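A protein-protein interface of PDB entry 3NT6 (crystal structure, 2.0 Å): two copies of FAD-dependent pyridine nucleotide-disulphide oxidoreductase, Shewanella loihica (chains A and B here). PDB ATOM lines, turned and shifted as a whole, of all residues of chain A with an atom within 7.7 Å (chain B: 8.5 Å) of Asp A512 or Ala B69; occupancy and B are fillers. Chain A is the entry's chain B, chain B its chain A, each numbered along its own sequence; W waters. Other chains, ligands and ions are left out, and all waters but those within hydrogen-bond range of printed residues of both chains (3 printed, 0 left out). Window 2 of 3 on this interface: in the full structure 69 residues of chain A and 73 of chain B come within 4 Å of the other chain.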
ATOM      1  N   VAL A 492     -14.638  27.440 -23.625  1.00  0.00           N
ATOM      2  CA  VAL A 492     -16.007  27.591 -24.206  1.00  0.00           C
ATOM      3  C   VAL A 492     -16.197  28.960 -24.897  1.00  0.00           C
ATOM      4  O   VAL A 492     -17.315  29.355 -25.277  1.00  0.00           O
ATOM      5  CB  VAL A 492     -17.099  27.340 -23.162  1.00  0.00           C
ATOM      6  CG1 VAL A 492     -16.997  25.957 -22.588  1.00  0.00           C
ATOM      7  CG2 VAL A 492     -17.005  28.325 -21.929  1.00  0.00           C
ATOM      8  N   ARG A 493     -15.099  29.654 -25.126  1.00  0.00           N
ATOM      9  CA  ARG A 493     -15.087  30.851 -25.995  1.00  0.00           C
ATOM     10  C   ARG A 493     -15.344  30.530 -27.441  1.00  0.00           C
ATOM     11  O   ARG A 493     -15.448  29.330 -27.845  1.00  0.00           O
ATOM     12  CB  ARG A 493     -13.782  31.687 -25.791  1.00  0.00           C
ATOM     13  CG  ARG A 493     -13.798  32.103 -24.329  1.00  0.00           C
ATOM     14  CD  ARG A 493     -12.471  32.782 -23.852  1.00  0.00           C
ATOM     15  NE  ARG A 493     -11.307  31.920 -24.233  1.00  0.00           N
ATOM     16  CZ  ARG A 493     -10.075  32.354 -24.514  1.00  0.00           C
ATOM     17  NH1 ARG A 493      -9.793  33.677 -24.535  1.00  0.00           N
ATOM     18  NH2 ARG A 493      -9.131  31.445 -24.778  1.00  0.00           N
ATOM     19  N   ASN A 494     -15.491  31.587 -28.225  1.00  0.00           N
ATOM     20  CA  ASN A 494     -15.740  31.451 -29.597  1.00  0.00           C
ATOM     21  C   ASN A 494     -14.356  31.322 -30.255  1.00  0.00           C
ATOM     22  O   ASN A 494     -13.388  31.892 -29.774  1.00  0.00           O
ATOM     23  CB  ASN A 494     -16.521  32.710 -30.076  1.00  0.00           C
ATOM     24  CG  ASN A 494     -18.032  32.452 -30.293  1.00  0.00           C
ATOM     25  OD1 ASN A 494     -18.577  32.792 -31.347  1.00  0.00           O
ATOM     26  ND2 ASN A 494     -18.671  31.798 -29.377  1.00  0.00           N
ATOM     27  N   ILE A 509     -15.134  23.891 -27.290  1.00  0.00           N
ATOM     28  CA  ILE A 509     -16.524  23.872 -27.749  1.00  0.00           C
ATOM     29  C   ILE A 509     -17.289  25.180 -27.262  1.00  0.00           C
ATOM     30  O   ILE A 509     -17.543  25.317 -26.037  1.00  0.00           O
ATOM     31  CB  ILE A 509     -17.239  22.601 -27.261  1.00  0.00           C
ATOM     32  CG1 ILE A 509     -16.494  21.253 -27.570  1.00  0.00           C
ATOM     33  CG2 ILE A 509     -18.649  22.556 -27.724  1.00  0.00           C
ATOM     34  CD1 ILE A 509     -17.160  20.031 -26.735  1.00  0.00           C
ATOM     35  N   PRO A 510     -17.681  26.087 -28.214  1.00  0.00           N
ATOM     36  CA  PRO A 510     -18.305  27.364 -27.831  1.00  0.00           C
ATOM     37  C   PRO A 510     -19.573  27.107 -27.080  1.00  0.00           C
ATOM     38  O   PRO A 510     -20.314  26.185 -27.416  1.00  0.00           O
ATOM     39  CB  PRO A 510     -18.630  28.010 -29.168  1.00  0.00           C
ATOM     40  CG  PRO A 510     -17.530  27.490 -30.080  1.00  0.00           C
ATOM     41  CD  PRO A 510     -17.350  26.051 -29.646  1.00  0.00           C
ATOM     42  N   VAL A 511     -19.862  27.904 -26.080  1.00  0.00           N
ATOM     43  CA  VAL A 511     -20.920  27.460 -25.195  1.00  0.00           C
ATOM     44  C   VAL A 511     -22.233  27.307 -25.950  1.00  0.00           C
ATOM     45  O   VAL A 511     -23.068  26.578 -25.517  1.00  0.00           O
ATOM     46  CB  VAL A 511     -21.377  28.455 -24.183  1.00  0.00           C
ATOM     47  CG1 VAL A 511     -21.497  27.922 -22.805  1.00  0.00           C
ATOM     48  CG2 VAL A 511     -21.086  29.891 -24.590  1.00  0.00           C
ATOM     49  N   ASP A 512     -22.410  28.037 -27.031  1.00  0.00           N
ATOM     50  CA  ASP A 512     -23.692  28.038 -27.738  1.00  0.00           C
ATOM     51  C   ASP A 512     -23.812  26.898 -28.684  1.00  0.00           C
ATOM     52  O   ASP A 512     -24.879  26.709 -29.264  1.00  0.00           O
ATOM     53  CB  ASP A 512     -23.983  29.381 -28.445  1.00  0.00           C
ATOM     54  CG  ASP A 512     -24.101  30.576 -27.431  1.00  0.00           C
ATOM     55  OD1 ASP A 512     -24.344  30.336 -26.204  1.00  0.00           O
ATOM     56  OD2 ASP A 512     -23.929  31.724 -27.878  1.00  0.00           O
ATOM     57  N   GLU A 513     -22.781  26.064 -28.750  1.00  0.00           N
ATOM     58  CA  GLU A 513     -22.887  24.832 -29.537  1.00  0.00           C
ATOM     59  C   GLU A 513     -22.743  23.613 -28.632  1.00  0.00           C
ATOM     60  O   GLU A 513     -22.838  22.446 -29.072  1.00  0.00           O
ATOM     61  CB  GLU A 513     -21.804  24.795 -30.601  1.00  0.00           C
ATOM     62  CG  GLU A 513     -21.580  26.128 -31.422  1.00  0.00           C
ATOM     63  CD  GLU A 513     -20.359  26.020 -32.422  1.00  0.00           C
ATOM     64  OE1 GLU A 513     -19.587  25.025 -32.322  1.00  0.00           O
ATOM     65  OE2 GLU A 513     -20.171  26.917 -33.288  1.00  0.00           O
ATOM     66  N   LEU A 514     -22.539  23.875 -27.357  1.00  0.00           N
ATOM     67  CA  LEU A 514     -22.267  22.819 -26.409  1.00  0.00           C
ATOM     68  C   LEU A 514     -23.399  21.880 -26.117  1.00  0.00           C
ATOM     69  O   LEU A 514     -23.144  20.715 -25.854  1.00  0.00           O
ATOM     70  CB  LEU A 514     -21.603  23.355 -25.126  1.00  0.00           C
ATOM     71  CG  LEU A 514     -21.244  22.401 -24.000  1.00  0.00           C
ATOM     72  CD1 LEU A 514     -19.935  21.594 -24.289  1.00  0.00           C
ATOM     73  CD2 LEU A 514     -21.163  23.131 -22.549  1.00  0.00           C
ATOM     74  N   ARG A 515     -24.649  22.321 -26.143  1.00  0.00           N
ATOM     75  CA  ARG A 515     -25.714  21.335 -25.763  1.00  0.00           C
ATOM     76  C   ARG A 515     -25.787  20.259 -26.876  1.00  0.00           C
ATOM     77  O   ARG A 515     -25.861  19.087 -26.597  1.00  0.00           O
ATOM     78  CB  ARG A 515     -27.046  22.030 -25.471  1.00  0.00           C
ATOM     79  CG  ARG A 515     -28.323  21.174 -25.299  1.00  0.00           C
ATOM     80  CD  ARG A 515     -29.507  22.125 -25.004  1.00  0.00           C
ATOM     81  NE  ARG A 515     -29.339  22.747 -23.664  1.00  0.00           N
ATOM     82  CZ  ARG A 515     -28.889  23.984 -23.464  1.00  0.00           C
ATOM     83  NH1 ARG A 515     -28.547  24.740 -24.525  1.00  0.00           N
ATOM     84  NH2 ARG A 515     -28.779  24.454 -22.246  1.00  0.00           N
ATOM     85  N   ASP A 516     -25.605  20.662 -28.123  1.00  0.00           N
ATOM     86  CA  ASP A 516     -25.656  19.708 -29.251  1.00  0.00           C
ATOM     87  C   ASP A 516     -24.382  18.859 -29.475  1.00  0.00           C
ATOM     88  O   ASP A 516     -24.438  17.838 -30.167  1.00  0.00           O
ATOM     89  CB  ASP A 516     -25.952  20.419 -30.580  1.00  0.00           C
ATOM     90  CG  ASP A 516     -27.250  21.282 -30.558  1.00  0.00           C
ATOM     91  OD1 ASP A 516     -28.248  20.932 -29.849  1.00  0.00           O
ATOM     92  OD2 ASP A 516     -27.231  22.310 -31.283  1.00  0.00           O
ATOM     93  N   ARG A 517     -23.257  19.274 -28.893  1.00  0.00           N
ATOM     94  CA  ARG A 517     -21.937  18.668 -29.217  1.00  0.00           C
ATOM     95  C   ARG A 517     -21.416  17.950 -28.010  1.00  0.00           C
ATOM     96  O   ARG A 517     -20.304  17.479 -28.022  1.00  0.00           O
ATOM     97  CB  ARG A 517     -20.902  19.723 -29.683  1.00  0.00           C
ATOM     98  CG  ARG A 517     -21.135  20.242 -31.109  1.00  0.00           C
ATOM     99  CD  ARG A 517     -20.112  21.312 -31.563  1.00  0.00           C
ATOM    100  NE  ARG A 517     -18.724  20.818 -31.468  1.00  0.00           N
ATOM    101  CZ  ARG A 517     -17.624  21.591 -31.521  1.00  0.00           C
ATOM    102  NH1 ARG A 517     -17.712  22.917 -31.708  1.00  0.00           N
ATOM    103  NH2 ARG A 517     -16.413  21.031 -31.413  1.00  0.00           N
ATOM    104  N   ARG A 536     -19.838  32.762 -19.306  1.00  0.00           N
ATOM    105  CA  ARG A 536     -20.148  31.645 -20.210  1.00  0.00           C
ATOM    106  C   ARG A 536     -19.658  30.283 -19.646  1.00  0.00           C
ATOM    107  O   ARG A 536     -20.347  29.237 -19.830  1.00  0.00           O
ATOM    108  CB  ARG A 536     -19.571  31.847 -21.585  1.00  0.00           C
ATOM    109  CG  ARG A 536     -20.325  32.847 -22.421  1.00  0.00           C
ATOM    110  CD  ARG A 536     -19.504  33.204 -23.586  1.00  0.00           C
ATOM    111  NE  ARG A 536     -18.241  33.904 -23.318  1.00  0.00           N
ATOM    112  CZ  ARG A 536     -17.308  34.130 -24.252  1.00  0.00           C
ATOM    113  NH1 ARG A 536     -17.430  33.636 -25.487  1.00  0.00           N
ATOM    114  NH2 ARG A 536     -16.253  34.852 -23.997  1.00  0.00           N
ATOM    115  N   VAL A 539     -22.434  28.932 -17.364  1.00  0.00           N
ATOM    116  CA  VAL A 539     -23.559  28.455 -18.167  1.00  0.00           C
ATOM    117  C   VAL A 539     -23.151  27.006 -18.572  1.00  0.00           C
ATOM    118  O   VAL A 539     -23.941  26.000 -18.393  1.00  0.00           O
ATOM    119  CB  VAL A 539     -23.850  29.351 -19.414  1.00  0.00           C
ATOM    120  CG1 VAL A 539     -24.842  28.609 -20.325  1.00  0.00           C
ATOM    121  CG2 VAL A 539     -24.378  30.818 -19.018  1.00  0.00           C
ATOM    122  N   GLN A 543     -24.822  23.217 -17.606  1.00  0.00           N
ATOM    123  CA  GLN A 543     -25.246  22.182 -18.548  1.00  0.00           C
ATOM    124  C   GLN A 543     -24.603  20.804 -18.303  1.00  0.00           C
ATOM    125  O   GLN A 543     -25.303  19.757 -18.370  1.00  0.00           O
ATOM    126  CB  GLN A 543     -24.927  22.575 -19.992  1.00  0.00           C
ATOM    127  CG  GLN A 543     -25.751  23.712 -20.552  1.00  0.00           C
ATOM    128  CD  GLN A 543     -25.346  23.817 -21.986  1.00  0.00           C
ATOM    129  OE1 GLN A 543     -24.945  22.806 -22.589  1.00  0.00           O
ATOM    130  NE2 GLN A 543     -25.422  24.980 -22.530  1.00  0.00           N
ATOM    131  N   ARG B  21     -33.180  27.227 -16.628  1.00  0.00           N
ATOM    132  CA  ARG B  21     -32.394  26.309 -17.420  1.00  0.00           C
ATOM    133  C   ARG B  21     -31.135  25.907 -16.593  1.00  0.00           C
ATOM    134  O   ARG B  21     -30.767  24.711 -16.556  1.00  0.00           O
ATOM    135  CB  ARG B  21     -31.983  26.978 -18.781  1.00  0.00           C
ATOM    136  CG  ARG B  21     -31.067  26.005 -19.689  1.00  0.00           C
ATOM    137  CD  ARG B  21     -31.791  24.531 -19.843  1.00  0.00           C
ATOM    138  NE  ARG B  21     -33.060  24.548 -20.679  1.00  0.00           N
ATOM    139  CZ  ARG B  21     -34.185  23.812 -20.484  1.00  0.00           C
ATOM    140  NH1 ARG B  21     -34.378  23.044 -19.422  1.00  0.00           N
ATOM    141  NH2 ARG B  21     -35.131  23.863 -21.347  1.00  0.00           N
ATOM    142  N   GLU B  25     -31.651  20.662 -16.708  1.00  0.00           N
ATOM    143  CA  GLU B  25     -31.651  20.465 -18.138  1.00  0.00           C
ATOM    144  C   GLU B  25     -32.918  19.756 -18.666  1.00  0.00           C
ATOM    145  O   GLU B  25     -33.140  19.804 -19.873  1.00  0.00           O
ATOM    146  CB  GLU B  25     -30.373  19.712 -18.603  1.00  0.00           C
ATOM    147  CG  GLU B  25     -29.083  20.702 -18.744  1.00  0.00           C
ATOM    148  CD  GLU B  25     -29.227  21.730 -19.922  1.00  0.00           C
ATOM    149  OE1 GLU B  25     -29.728  21.350 -20.998  1.00  0.00           O
ATOM    150  OE2 GLU B  25     -28.881  22.956 -19.761  1.00  0.00           O
ATOM    151  N   GLN B  62     -30.693  39.789 -26.545  1.00  0.00           N
ATOM    152  CA  GLN B  62     -30.757  38.392 -26.912  1.00  0.00           C
ATOM    153  C   GLN B  62     -31.729  38.333 -28.062  1.00  0.00           C
ATOM    154  O   GLN B  62     -32.435  39.301 -28.337  1.00  0.00           O
ATOM    155  CB  GLN B  62     -31.319  37.570 -25.757  1.00  0.00           C
ATOM    156  CG  GLN B  62     -30.490  37.572 -24.474  1.00  0.00           C
ATOM    157  CD  GLN B  62     -29.225  36.775 -24.619  1.00  0.00           C
ATOM    158  OE1 GLN B  62     -29.071  35.994 -25.543  1.00  0.00           O
ATOM    159  NE2 GLN B  62     -28.263  37.016 -23.712  1.00  0.00           N
ATOM    160  N   THR B  63     -31.731  37.204 -28.782  1.00  0.00           N
ATOM    161  CA  THR B  63     -32.766  36.907 -29.781  1.00  0.00           C
ATOM    162  C   THR B  63     -33.464  35.592 -29.458  1.00  0.00           C
ATOM    163  O   THR B  63     -32.973  34.842 -28.618  1.00  0.00           O
ATOM    164  CB  THR B  63     -32.169  36.852 -31.204  1.00  0.00           C
ATOM    165  OG1 THR B  63     -31.477  35.617 -31.356  1.00  0.00           O
ATOM    166  CG2 THR B  63     -31.183  37.996 -31.447  1.00  0.00           C
ATOM    167  N   PRO B  64     -34.643  35.290 -30.113  1.00  0.00           N
ATOM    168  CA  PRO B  64     -35.219  33.959 -29.990  1.00  0.00           C
ATOM    169  C   PRO B  64     -34.124  32.921 -30.284  1.00  0.00           C
ATOM    170  O   PRO B  64     -33.989  31.902 -29.565  1.00  0.00           O
ATOM    171  CB  PRO B  64     -36.305  33.903 -31.099  1.00  0.00           C
ATOM    172  CG  PRO B  64     -36.723  35.390 -31.271  1.00  0.00           C
ATOM    173  CD  PRO B  64     -35.536  36.264 -30.785  1.00  0.00           C
ATOM    174  N   GLU B  65     -33.363  33.133 -31.344  1.00  0.00           N
ATOM    175  CA  GLU B  65     -32.346  32.132 -31.725  1.00  0.00           C
ATOM    176  C   GLU B  65     -31.239  31.957 -30.638  1.00  0.00           C
ATOM    177  O   GLU B  65     -30.848  30.830 -30.340  1.00  0.00           O
ATOM    178  CB  GLU B  65     -31.704  32.497 -33.117  1.00  0.00           C
ATOM    179  CG  GLU B  65     -32.697  32.378 -34.304  1.00  0.00           C
ATOM    180  CD  GLU B  65     -33.650  33.594 -34.496  1.00  0.00           C
ATOM    181  OE1 GLU B  65     -33.487  34.658 -33.886  1.00  0.00           O
ATOM    182  OE2 GLU B  65     -34.562  33.495 -35.346  1.00  0.00           O
ATOM    183  N   SER B  66     -30.681  33.053 -30.139  1.00  0.00           N
ATOM    184  CA  SER B  66     -29.623  33.048 -29.089  1.00  0.00           C
ATOM    185  C   SER B  66     -30.141  32.431 -27.699  1.00  0.00           C
ATOM    186  O   SER B  66     -29.488  31.609 -27.031  1.00  0.00           O
ATOM    187  CB  SER B  66     -29.105  34.496 -28.943  1.00  0.00           C
ATOM    188  OG  SER B  66     -30.008  35.252 -28.123  1.00  0.00           O
ATOM    189  N   PHE B  67     -31.361  32.758 -27.316  1.00  0.00           N
ATOM    190  CA  PHE B  67     -32.079  31.985 -26.255  1.00  0.00           C
ATOM    191  C   PHE B  67     -32.275  30.469 -26.504  1.00  0.00           C
ATOM    192  O   PHE B  67     -32.105  29.659 -25.606  1.00  0.00           O
ATOM    193  CB  PHE B  67     -33.451  32.600 -25.967  1.00  0.00           C
ATOM    194  CG  PHE B  67     -33.516  33.326 -24.713  1.00  0.00           C
ATOM    195  CD1 PHE B  67     -33.785  34.710 -24.703  1.00  0.00           C
ATOM    196  CD2 PHE B  67     -33.325  32.641 -23.489  1.00  0.00           C
ATOM    197  CE1 PHE B  67     -33.884  35.385 -23.511  1.00  0.00           C
ATOM    198  CE2 PHE B  67     -33.323  33.353 -22.243  1.00  0.00           C
ATOM    199  CZ  PHE B  67     -33.573  34.706 -22.257  1.00  0.00           C
ATOM    200  N   LYS B  68     -32.599  30.042 -27.723  1.00  0.00           N
ATOM    201  CA  LYS B  68     -32.556  28.595 -28.037  1.00  0.00           C
ATOM    202  C   LYS B  68     -31.146  27.966 -27.944  1.00  0.00           C
ATOM    203  O   LYS B  68     -31.006  26.823 -27.510  1.00  0.00           O
ATOM    204  CB  LYS B  68     -33.088  28.352 -29.434  1.00  0.00           C
ATOM    205  CG  LYS B  68     -33.136  26.841 -29.898  1.00  0.00           C
ATOM    206  CD  LYS B  68     -34.555  26.499 -30.171  1.00  0.00           C
ATOM    207  CE  LYS B  68     -34.917  25.046 -29.740  1.00  0.00           C
ATOM    208  NZ  LYS B  68     -36.438  24.839 -29.866  1.00  0.00           N
ATOM    209  N   ALA B  69     -30.119  28.683 -28.365  1.00  0.00           N
ATOM    210  CA  ALA B  69     -28.803  28.045 -28.628  1.00  0.00           C
ATOM    211  C   ALA B  69     -28.104  27.917 -27.255  1.00  0.00           C
ATOM    212  O   ALA B  69     -27.664  26.771 -26.853  1.00  0.00           O
ATOM    213  CB  ALA B  69     -27.940  28.875 -29.635  1.00  0.00           C
ATOM    214  N   ARG B  70     -28.158  29.028 -26.498  1.00  0.00           N
ATOM    215  CA  ARG B  70     -27.624  29.099 -25.164  1.00  0.00           C
ATOM    216  C   ARG B  70     -28.477  28.284 -24.105  1.00  0.00           C
ATOM    217  O   ARG B  70     -27.956  27.422 -23.440  1.00  0.00           O
ATOM    218  CB  ARG B  70     -27.428  30.560 -24.676  1.00  0.00           C
ATOM    219  CG  ARG B  70     -26.599  30.540 -23.362  1.00  0.00           C
ATOM    220  CD  ARG B  70     -25.802  31.786 -23.059  1.00  0.00           C
ATOM    221  NE  ARG B  70     -24.805  32.108 -24.069  1.00  0.00           N
ATOM    222  CZ  ARG B  70     -23.961  33.145 -23.982  1.00  0.00           C
ATOM    223  NH1 ARG B  70     -24.096  33.991 -22.943  1.00  0.00           N
ATOM    224  NH2 ARG B  70     -23.097  33.378 -24.960  1.00  0.00           N
ATOM    225  N   PHE B  71     -29.752  28.639 -23.944  1.00  0.00           N
ATOM    226  CA  PHE B  71     -30.557  28.141 -22.913  1.00  0.00           C
ATOM    227  C   PHE B  71     -31.577  27.057 -23.331  1.00  0.00           C
ATOM    228  O   PHE B  71     -32.354  26.642 -22.500  1.00  0.00           O
ATOM    229  CB  PHE B  71     -31.204  29.369 -22.159  1.00  0.00           C
ATOM    230  CG  PHE B  71     -30.195  30.155 -21.439  1.00  0.00           C
ATOM    231  CD1 PHE B  71     -29.466  29.554 -20.407  1.00  0.00           C
ATOM    232  CD2 PHE B  71     -29.915  31.459 -21.787  1.00  0.00           C
ATOM    233  CE1 PHE B  71     -28.482  30.297 -19.668  1.00  0.00           C
ATOM    234  CE2 PHE B  71     -28.924  32.190 -21.107  1.00  0.00           C
ATOM    235  CZ  PHE B  71     -28.230  31.640 -20.060  1.00  0.00           C
ATOM    236  N   ASN B  72     -31.582  26.566 -24.592  1.00  0.00           N
ATOM    237  CA  ASN B  72     -32.699  25.703 -24.998  1.00  0.00           C
ATOM    238  C   ASN B  72     -34.090  26.123 -24.391  1.00  0.00           C
ATOM    239  O   ASN B  72     -34.903  25.275 -23.886  1.00  0.00           O
ATOM    240  CB  ASN B  72     -32.420  24.247 -24.571  1.00  0.00           C
ATOM    241  CG  ASN B  72     -33.316  23.244 -25.339  1.00  0.00           C
ATOM    242  OD1 ASN B  72     -33.612  23.438 -26.558  1.00  0.00           O
ATOM    243  ND2 ASN B  72     -33.741  22.187 -24.653  1.00  0.00           N
ATOM    244  N   VAL B  73     -34.367  27.418 -24.428  1.00  0.00           N
ATOM    245  CA  VAL B  73     -35.694  27.984 -24.183  1.00  0.00           C
ATOM    246  C   VAL B  73     -36.419  28.338 -25.497  1.00  0.00           C
ATOM    247  O   VAL B  73     -35.900  29.143 -26.272  1.00  0.00           O
ATOM    248  CB  VAL B  73     -35.535  29.231 -23.347  1.00  0.00           C
ATOM    249  CG1 VAL B  73     -36.844  29.968 -23.126  1.00  0.00           C
ATOM    250  CG2 VAL B  73     -34.879  28.844 -21.958  1.00  0.00           C
ATOM    251  N   GLU B  74     -37.615  27.757 -25.753  1.00  0.00           N
ATOM    252  CA  GLU B  74     -38.403  28.150 -26.914  1.00  0.00           C
ATOM    253  C   GLU B  74     -39.108  29.498 -26.619  1.00  0.00           C
ATOM    254  O   GLU B  74     -39.943  29.638 -25.699  1.00  0.00           O
ATOM    255  CB  GLU B  74     -39.457  27.140 -27.189  1.00  0.00           C
ATOM    256  CG  GLU B  74     -39.762  27.137 -28.621  1.00  0.00           C
ATOM    257  CD  GLU B  74     -41.140  26.524 -28.895  1.00  0.00           C
ATOM    258  OE1 GLU B  74     -41.642  25.766 -28.004  1.00  0.00           O
ATOM    259  OE2 GLU B  74     -41.691  26.805 -29.980  1.00  0.00           O
HETATM  260  O   HOH W   1     -29.173  24.381 -27.469  1.00  0.00           O
HETATM  261  O   HOH W   2     -27.444  26.415 -20.818  1.00  0.00           O
HETATM  262  O   HOH W   3     -25.544  25.106 -25.766  1.00  0.00           O
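Of chain B, only Ala B69 (3.7 Å) and Arg B70 (2.8 Å) come within 4 Å of Asp A512. Printed residues of chain A within 4 Å of Ala B69: Asp A512 (3.7 Å) and Arg A515 (3.2 Å). No residue of chain B comes within 4 Å of Val A511. Of the printed residues of chain A, Arg B21 touches Arg A515 (3.8 Å). Printed residues of chain B within 4 Å of Gln A543: Glu B25 (3.3 Å) and Arg B70 (3.6 Å). Printed residues of chain A within 4 Å of Arg B70: Asp A512 (2.8 Å), Arg A515 (3.0 Å), Arg A536 (3.8 Å) and Gln A543 (3.6 Å). Printed residues of chain A within 4 Å of Asn B72: Arg A515. Printed residues of chain B within 4 Å of Arg A536: Arg B70 (3.8 Å). The nearest residue of chain B that does not touch Asp A512 is Ser B66 (5.4 Å). The nearest residue of chain A that does not touch Ala B69 is Val A511 (4.8 Å). The nearest printed residue of chain B that does not touch Arg A536 is Phe B71 (8.1 Å).
The backbone NH (N) of Asn B72 lies within hydrogen-bond range of the backbone carbonyl oxygen (O) of Phe B67 (3.3 Å). The guanidinium group of Arg B21 is in hydrogen-bond range of the backbone carbonyl oxygen of Glu B25 (3.5 Å). The guanidinium group (NH2) of Arg A515 sits close to the side-chain amide nitrogen (NE2) of Gln A543, 3.4 Å away. The guanidinium group of Arg B21 is in hydrogen-bond range of the backbone carbonyl oxygen of Phe B71. The guanidinium group (NH2) of Arg B21 is in hydrogen-bond range of the backbone carbonyl oxygen (O) of Asn B72, 2.9 Å away.
Printed residues of chain A that touch a printed residue of chain B: Asp A512, Arg A515, Arg A536 and Gln A543. Among the printed residues, Asp or Glu carboxylates within 4 Å of a Lys or Arg side-chain nitrogen of the other chain: Asp A512 with Arg B70 (2.8 Å) and Arg A515 with Glu B25 (2.9 Å).
OE2 of Glu B25 lies within salt-bridge range of NH2 of Arg A515, 2.9 Å away. The guanidinium group (NE) of Arg B70 lies within salt-bridge range of the side-chain carboxylate (OD1) of Asp A512, 2.8 Å away. The guanidinium group of Arg A515 sits at hydrogen-bond distance from the backbone carbonyl oxygen of Ala B69 (3.2 Å). O of Arg B70 is in hydrogen-bond range of NH1 of Arg A515, 3.0 Å away.
No position is printed for both chains. Of the 11 pairs that touch across the chains among the printed residues, none has its exchanged pair printed and touching as well.
Asp A512 touches Ala B69 (O to O, 3.7 Å). Arg B21 touches Arg A515. NH2 of Arg A515 touches C of Phe B71, at 3.97 Å. Arg A515 touches Asn B72. NH2 of Arg B70 touches CG of Arg A536 (3.8 Å). Gln A543 touches Glu B25. NE2 of Gln A543 touches O of Arg B70 (3.6 Å).
Water W2 lies within hydrogen-bond range of NH2 of Arg A515, O of Arg B70 and NE2 of Gln A543. Water W3 lies within hydrogen-bond range of the backbone carbonyl oxygen (O) of Val A511, the backbone carbonyl oxygen (O) of Ala B69, the backbone NH (N) of Arg A515 and the side-chain amide nitrogen (NE2) of Gln A543. Water W1 lies within hydrogen-bond range of the backbone carbonyl oxygen of Ala B69 (2.9 Å), the guanidinium group of Arg A515 (3.0 Å) and the backbone carbonyl oxygen of Lys B68 (3.1 Å).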
